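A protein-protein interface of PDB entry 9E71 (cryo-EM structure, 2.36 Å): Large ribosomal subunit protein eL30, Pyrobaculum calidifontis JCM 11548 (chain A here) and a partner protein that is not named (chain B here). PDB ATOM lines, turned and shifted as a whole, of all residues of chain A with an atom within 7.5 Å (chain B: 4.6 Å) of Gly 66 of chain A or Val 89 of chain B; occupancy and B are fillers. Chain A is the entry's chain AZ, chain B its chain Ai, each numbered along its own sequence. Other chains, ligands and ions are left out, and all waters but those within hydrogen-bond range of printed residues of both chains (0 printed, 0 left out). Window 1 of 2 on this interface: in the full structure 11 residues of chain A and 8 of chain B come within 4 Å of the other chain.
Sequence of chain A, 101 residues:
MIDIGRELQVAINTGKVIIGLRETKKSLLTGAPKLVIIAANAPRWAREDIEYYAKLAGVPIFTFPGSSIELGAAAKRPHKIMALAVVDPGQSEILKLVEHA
NH1 of Arg 44 of chain B lies within salt-bridge range of OE2 of Glu 90 of chain B (3.4 Å). The side-chain hydroxyl (OG) of Ser 67 of chain A lies close to the backbone NH (N) of Ile 69 of chain A (3.4 Å). OD1 of Asn 41 of chain A sits at hydrogen-bond distance from N of Ser 68 of chain A, at 2.7 Å. The side-chain carboxylate of Glu 70 of chain A sits at hydrogen-bond distance from the backbone NH of Ser 67 of chain A, 3.1 Å away. The backbone NH of Ala 40 of chain A is in hydrogen-bond range of the backbone carbonyl oxygen of Gly 66 of chain A, 2.9 Å away.
Among the printed residues, pairs that only touch across the chains: Pro 65 of chain A with Lys 93 of chain B, Thr 63 of chain A with Glu 92 of chain B, Asn 41 of chain A with Val 89 of chain B, Gly 66 of chain A with Val 89 of chain B, Ala 40 of chain A with Glu 92 of chain B, Pro 65 of chain A with Val 89 of chain B, Asn 41 of chain A with Arg 44 of chain B, Ala 40 of chain A with Val 89 of chain B, Pro 65 of chain A with Glu 92 of chain B and Ser 67 of chain A with Val 89 of chain B.
OE1 of Glu 70 of chain A is in salt-bridge range of NZ of Lys 93 of chain B (3.7 Å).
Of the printed residues of chain B, Pro 65 of chain A touches Val 89 (3.6 Å), Glu 92 (3.7 Å) and Lys 93 (3.3 Å). Gly 66 of chain A touches just one residue of chain B: Val 89. Ile 81 of chain A touches none of the printed residues of chain B. Of the printed residues of chain A, Val 89 of chain B touches Ala 40 (3.6 Å), Asn 41 (3.4 Å), Pro 65 (3.6 Å), Gly 66 (3.5 Å) and Ser 67 (3.9 Å). Printed residues of chain A within 4 Å of Lys 93 of chain B: Pro 65 and Glu 70. The nearest residue of chain A that does not touch Val 89 of chain B is Glu 70 of chain A (4.6 Å).
Hydrophobic or aromatic side chains of chain A within 4 Å of the printed part of chain B: Ala 40 and Pro 65. Printed residues of chain B that touch a printed residue of chain A: Arg 44, Val 89, Glu 92 and Lys 93. Among the printed residues, 11 pairs touch across the chains. Among the printed residues, Asp or Glu carboxylates within 4 Å of a Lys or Arg side-chain nitrogen of the other chain: Glu 70 of chain A with Lys 93 of chain B.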
ATOM      1  N   ILE A  38      -1.153 -11.430  19.340  1.00  0.00           N
ATOM      2  CA  ILE A  38      -0.201 -11.653  20.424  1.00  0.00           C
ATOM      3  C   ILE A  38       1.164 -11.132  19.993  1.00  0.00           C
ATOM      4  O   ILE A  38       1.565 -11.307  18.840  1.00  0.00           O
ATOM      5  CB  ILE A  38      -0.129 -13.139  20.823  1.00  0.00           C
ATOM      6  CG1 ILE A  38       0.548 -13.291  22.184  1.00  0.00           C
ATOM      7  CG2 ILE A  38       0.608 -13.960  19.782  1.00  0.00           C
ATOM      8  CD1 ILE A  38       0.373 -14.647  22.794  1.00  0.00           C
ATOM      9  N   ALA A  39       1.864 -10.475  20.912  1.00  0.00           N
ATOM     10  CA  ALA A  39       3.189  -9.961  20.595  1.00  0.00           C
ATOM     11  C   ALA A  39       4.176 -11.105  20.403  1.00  0.00           C
ATOM     12  O   ALA A  39       4.070 -12.161  21.033  1.00  0.00           O
ATOM     13  CB  ALA A  39       3.679  -9.023  21.695  1.00  0.00           C
ATOM     14  N   ALA A  40       5.142 -10.885  19.510  1.00  0.00           N
ATOM     15  CA  ALA A  40       6.084 -11.941  19.158  1.00  0.00           C
ATOM     16  C   ALA A  40       7.007 -12.292  20.316  1.00  0.00           C
ATOM     17  O   ALA A  40       7.442 -13.442  20.429  1.00  0.00           O
ATOM     18  CB  ALA A  40       6.903 -11.529  17.939  1.00  0.00           C
ATOM     19  N   ASN A  41       7.324 -11.326  21.175  1.00  0.00           N
ATOM     20  CA  ASN A  41       8.201 -11.560  22.315  1.00  0.00           C
ATOM     21  C   ASN A  41       7.423 -11.881  23.583  1.00  0.00           C
ATOM     22  O   ASN A  41       7.931 -11.677  24.691  1.00  0.00           O
ATOM     23  CB  ASN A  41       9.113 -10.356  22.540  1.00  0.00           C
ATOM     24  CG  ASN A  41       8.373  -9.164  23.102  1.00  0.00           C
ATOM     25  OD1 ASN A  41       7.197  -8.957  22.815  1.00  0.00           O
ATOM     26  ND2 ASN A  41       9.061  -8.373  23.914  1.00  0.00           N
ATOM     27  N   ALA A  42       6.201 -12.379  23.445  1.00  0.00           N
ATOM     28  CA  ALA A  42       5.410 -12.720  24.612  1.00  0.00           C
ATOM     29  C   ALA A  42       6.030 -13.911  25.338  1.00  0.00           C
ATOM     30  O   ALA A  42       6.655 -14.772  24.715  1.00  0.00           O
ATOM     31  CB  ALA A  42       3.973 -13.041  24.219  1.00  0.00           C
ATOM     32  N   PHE A  62      -3.187 -14.090  15.420  1.00  0.00           N
ATOM     33  CA  PHE A  62      -2.126 -13.506  14.626  1.00  0.00           C
ATOM     34  C   PHE A  62      -0.978 -13.125  15.546  1.00  0.00           C
ATOM     35  O   PHE A  62      -1.190 -12.533  16.610  1.00  0.00           O
ATOM     36  CB  PHE A  62      -2.622 -12.272  13.872  1.00  0.00           C
ATOM     37  CG  PHE A  62      -1.551 -11.560  13.102  1.00  0.00           C
ATOM     38  CD1 PHE A  62      -1.032 -12.106  11.944  1.00  0.00           C
ATOM     39  CD2 PHE A  62      -1.060 -10.347  13.540  1.00  0.00           C
ATOM     40  CE1 PHE A  62      -0.045 -11.453  11.238  1.00  0.00           C
ATOM     41  CE2 PHE A  62      -0.072  -9.690  12.839  1.00  0.00           C
ATOM     42  CZ  PHE A  62       0.435 -10.244  11.686  1.00  0.00           C
ATOM     43  N   THR A  63       0.233 -13.487  15.143  1.00  0.00           N
ATOM     44  CA  THR A  63       1.441 -13.104  15.857  1.00  0.00           C
ATOM     45  C   THR A  63       1.935 -11.796  15.260  1.00  0.00           C
ATOM     46  O   THR A  63       2.335 -11.752  14.093  1.00  0.00           O
ATOM     47  CB  THR A  63       2.507 -14.190  15.765  1.00  0.00           C
ATOM     48  OG1 THR A  63       2.114 -15.313  16.563  1.00  0.00           O
ATOM     49  CG2 THR A  63       3.842 -13.663  16.259  1.00  0.00           C
ATOM     50  N   PHE A  64       1.880 -10.735  16.055  1.00  0.00           N
ATOM     51  CA  PHE A  64       2.369  -9.440  15.621  1.00  0.00           C
ATOM     52  C   PHE A  64       3.863  -9.533  15.332  1.00  0.00           C
ATOM     53  O   PHE A  64       4.592 -10.215  16.058  1.00  0.00           O
ATOM     54  CB  PHE A  64       2.098  -8.391  16.700  1.00  0.00           C
ATOM     55  CG  PHE A  64       2.422  -6.994  16.282  1.00  0.00           C
ATOM     56  CD1 PHE A  64       1.600  -6.307  15.411  1.00  0.00           C
ATOM     57  CD2 PHE A  64       3.556  -6.367  16.757  1.00  0.00           C
ATOM     58  CE1 PHE A  64       1.907  -5.022  15.027  1.00  0.00           C
ATOM     59  CE2 PHE A  64       3.870  -5.087  16.372  1.00  0.00           C
ATOM     60  CZ  PHE A  64       3.043  -4.412  15.508  1.00  0.00           C
ATOM     61  N   PRO A  65       4.354  -8.869  14.286  1.00  0.00           N
ATOM     62  CA  PRO A  65       5.760  -9.046  13.895  1.00  0.00           C
ATOM     63  C   PRO A  65       6.743  -8.214  14.707  1.00  0.00           C
ATOM     64  O   PRO A  65       7.889  -8.022  14.291  1.00  0.00           O
ATOM     65  CB  PRO A  65       5.769  -8.635  12.418  1.00  0.00           C
ATOM     66  CG  PRO A  65       4.589  -7.780  12.236  1.00  0.00           C
ATOM     67  CD  PRO A  65       3.598  -8.061  13.317  1.00  0.00           C
ATOM     68  N   GLY A  66       6.309  -7.711  15.858  1.00  0.00           N
ATOM     69  CA  GLY A  66       7.183  -7.010  16.771  1.00  0.00           C
ATOM     70  C   GLY A  66       7.059  -7.454  18.213  1.00  0.00           C
ATOM     71  O   GLY A  66       6.557  -8.542  18.501  1.00  0.00           O
ATOM     72  N   SER A  67       7.526  -6.614  19.129  1.00  0.00           N
ATOM     73  CA  SER A  67       7.487  -6.919  20.546  1.00  0.00           C
ATOM     74  C   SER A  67       6.248  -6.301  21.183  1.00  0.00           C
ATOM     75  O   SER A  67       5.404  -5.706  20.511  1.00  0.00           O
ATOM     76  CB  SER A  67       8.757  -6.418  21.228  1.00  0.00           C
ATOM     77  OG  SER A  67       8.779  -5.004  21.282  1.00  0.00           O
ATOM     78  N   SER A  68       6.142  -6.443  22.507  1.00  0.00           N
ATOM     79  CA  SER A  68       5.053  -5.813  23.244  1.00  0.00           C
ATOM     80  C   SER A  68       5.112  -4.296  23.124  1.00  0.00           C
ATOM     81  O   SER A  68       4.077  -3.634  22.965  1.00  0.00           O
ATOM     82  CB  SER A  68       5.116  -6.229  24.710  1.00  0.00           C
ATOM     83  OG  SER A  68       4.333  -7.381  24.947  1.00  0.00           O
ATOM     84  N   ILE A  69       6.320  -3.731  23.188  1.00  0.00           N
ATOM     85  CA  ILE A  69       6.477  -2.283  23.117  1.00  0.00           C
ATOM     86  C   ILE A  69       6.048  -1.760  21.756  1.00  0.00           C
ATOM     87  O   ILE A  69       5.303  -0.780  21.663  1.00  0.00           O
ATOM     88  CB  ILE A  69       7.929  -1.888  23.436  1.00  0.00           C
ATOM     89  CG1 ILE A  69       8.537  -2.856  24.445  1.00  0.00           C
ATOM     90  CG2 ILE A  69       7.982  -0.473  23.957  1.00  0.00           C
ATOM     91  CD1 ILE A  69       8.804  -2.237  25.787  1.00  0.00           C
ATOM     92  N   GLU A  70       6.494  -2.409  20.679  1.00  0.00           N
ATOM     93  CA  GLU A  70       6.122  -1.929  19.355  1.00  0.00           C
ATOM     94  C   GLU A  70       4.668  -2.227  19.028  1.00  0.00           C
ATOM     95  O   GLU A  70       4.056  -1.492  18.251  1.00  0.00           O
ATOM     96  CB  GLU A  70       7.058  -2.498  18.288  1.00  0.00           C
ATOM     97  CG  GLU A  70       8.493  -2.662  18.757  1.00  0.00           C
ATOM     98  CD  GLU A  70       9.227  -3.774  18.040  1.00  0.00           C
ATOM     99  OE1 GLU A  70       8.608  -4.435  17.192  1.00  0.00           O
ATOM    100  OE2 GLU A  70      10.425  -3.979  18.312  1.00  0.00           O
ATOM    101  N   LEU A  71       4.087  -3.273  19.616  1.00  0.00           N
ATOM    102  CA  LEU A  71       2.647  -3.463  19.485  1.00  0.00           C
ATOM    103  C   LEU A  71       1.885  -2.315  20.132  1.00  0.00           C
ATOM    104  O   LEU A  71       0.934  -1.780  19.546  1.00  0.00           O
ATOM    105  CB  LEU A  71       2.230  -4.795  20.100  1.00  0.00           C
ATOM    106  CG  LEU A  71       0.730  -5.086  20.061  1.00  0.00           C
ATOM    107  CD1 LEU A  71       0.190  -4.884  18.661  1.00  0.00           C
ATOM    108  CD2 LEU A  71       0.439  -6.493  20.554  1.00  0.00           C
ATOM    109  N   ILE A  81       1.871  -3.907  25.322  1.00  0.00           N
ATOM    110  CA  ILE A  81       0.691  -4.724  25.069  1.00  0.00           C
ATOM    111  C   ILE A  81       1.147  -6.131  24.714  1.00  0.00           C
ATOM    112  O   ILE A  81       1.699  -6.347  23.632  1.00  0.00           O
ATOM    113  CB  ILE A  81      -0.181  -4.153  23.945  1.00  0.00           C
ATOM    114  CG1 ILE A  81      -0.861  -2.862  24.389  1.00  0.00           C
ATOM    115  CG2 ILE A  81      -1.209  -5.168  23.510  1.00  0.00           C
ATOM    116  CD1 ILE A  81      -1.596  -2.175  23.278  1.00  0.00           C
ATOM    117  N   ARG B  44      12.628  -6.660  26.256  1.00  0.00           N
ATOM    118  CA  ARG B  44      13.094  -5.548  25.429  1.00  0.00           C
ATOM    119  C   ARG B  44      12.870  -4.189  26.082  1.00  0.00           C
ATOM    120  O   ARG B  44      12.839  -3.166  25.395  1.00  0.00           O
ATOM    121  CB  ARG B  44      12.440  -5.574  24.046  1.00  0.00           C
ATOM    122  CG  ARG B  44      12.306  -6.955  23.461  1.00  0.00           C
ATOM    123  CD  ARG B  44      13.085  -7.079  22.183  1.00  0.00           C
ATOM    124  NE  ARG B  44      13.367  -8.470  21.867  1.00  0.00           N
ATOM    125  CZ  ARG B  44      13.793  -8.895  20.687  1.00  0.00           C
ATOM    126  NH1 ARG B  44      13.992  -8.059  19.684  1.00  0.00           N
ATOM    127  NH2 ARG B  44      14.021 -10.192  20.509  1.00  0.00           N
ATOM    128  N   LYS B  87      15.041 -14.604  19.996  1.00  0.00           N
ATOM    129  CA  LYS B  87      14.961 -13.908  18.713  1.00  0.00           C
ATOM    130  C   LYS B  87      13.737 -14.377  17.929  1.00  0.00           C
ATOM    131  O   LYS B  87      13.828 -14.814  16.783  1.00  0.00           O
ATOM    132  CB  LYS B  87      16.241 -14.114  17.913  1.00  0.00           C
ATOM    133  CG  LYS B  87      16.794 -15.510  17.993  1.00  0.00           C
ATOM    134  CD  LYS B  87      17.859 -15.744  16.929  1.00  0.00           C
ATOM    135  CE  LYS B  87      19.209 -15.207  17.369  1.00  0.00           C
ATOM    136  NZ  LYS B  87      20.303 -16.191  17.137  1.00  0.00           N
ATOM    137  N   GLY B  88      12.580 -14.298  18.577  1.00  0.00           N
ATOM    138  CA  GLY B  88      11.330 -14.611  17.916  1.00  0.00           C
ATOM    139  C   GLY B  88      10.751 -13.408  17.204  1.00  0.00           C
ATOM    140  O   GLY B  88      10.101 -13.541  16.162  1.00  0.00           O
ATOM    141  N   VAL B  89      10.998 -12.221  17.761  1.00  0.00           N
ATOM    142  CA  VAL B  89      10.506 -10.988  17.156  1.00  0.00           C
ATOM    143  C   VAL B  89      11.151 -10.764  15.796  1.00  0.00           C
ATOM    144  O   VAL B  89      10.481 -10.389  14.827  1.00  0.00           O
ATOM    145  CB  VAL B  89      10.756  -9.796  18.095  1.00  0.00           C
ATOM    146  CG1 VAL B  89      10.701  -8.501  17.315  1.00  0.00           C
ATOM    147  CG2 VAL B  89       9.745  -9.786  19.217  1.00  0.00           C
ATOM    148  N   GLU B  90      12.462 -10.987  15.703  1.00  0.00           N
ATOM    149  CA  GLU B  90      13.154 -10.796  14.433  1.00  0.00           C
ATOM    150  C   GLU B  90      12.705 -11.819  13.397  1.00  0.00           C
ATOM    151  O   GLU B  90      12.574 -11.491  12.212  1.00  0.00           O
ATOM    152  CB  GLU B  90      14.663 -10.859  14.649  1.00  0.00           C
ATOM    153  CG  GLU B  90      15.148  -9.989  15.799  1.00  0.00           C
ATOM    154  CD  GLU B  90      15.005  -8.505  15.508  1.00  0.00           C
ATOM    155  OE1 GLU B  90      14.845  -8.144  14.322  1.00  0.00           O
ATOM    156  OE2 GLU B  90      15.051  -7.701  16.462  1.00  0.00           O
ATOM    157  N   ALA B  91      12.459 -13.061  13.823  1.00  0.00           N
ATOM    158  CA  ALA B  91      11.954 -14.070  12.898  1.00  0.00           C
ATOM    159  C   ALA B  91      10.562 -13.710  12.391  1.00  0.00           C
ATOM    160  O   ALA B  91      10.254 -13.899  11.207  1.00  0.00           O
ATOM    161  CB  ALA B  91      11.941 -15.438  13.575  1.00  0.00           C
ATOM    162  N   GLU B  92       9.707 -13.193  13.278  1.00  0.00           N
ATOM    163  CA  GLU B  92       8.388 -12.728  12.861  1.00  0.00           C
ATOM    164  C   GLU B  92       8.497 -11.569  11.880  1.00  0.00           C
ATOM    165  O   GLU B  92       7.741 -11.503  10.903  1.00  0.00           O
ATOM    166  CB  GLU B  92       7.568 -12.307  14.081  1.00  0.00           C
ATOM    167  CG  GLU B  92       6.945 -13.409  14.968  1.00  0.00           C
ATOM    168  CD  GLU B  92       6.514 -14.714  14.286  1.00  0.00           C
ATOM    169  OE1 GLU B  92       6.309 -14.775  13.056  1.00  0.00           O
ATOM    170  OE2 GLU B  92       6.383 -15.719  15.017  1.00  0.00           O
ATOM    171  N   LYS B  93       9.425 -10.642  12.133  1.00  0.00           N
ATOM    172  CA  LYS B  93       9.652  -9.531  11.213  1.00  0.00           C
ATOM    173  C   LYS B  93      10.086 -10.031   9.844  1.00  0.00           C
ATOM    174  O   LYS B  93       9.627  -9.526   8.814  1.00  0.00           O
ATOM    175  CB  LYS B  93      10.709  -8.585  11.781  1.00  0.00           C
ATOM    176  CG  LYS B  93      10.229  -7.175  12.067  1.00  0.00           C
ATOM    177  CD  LYS B  93      11.138  -6.499  13.078  1.00  0.00           C
ATOM    178  CE  LYS B  93      10.464  -5.310  13.730  1.00  0.00           C
ATOM    179  NZ  LYS B  93      11.371  -4.638  14.696  1.00  0.00           N
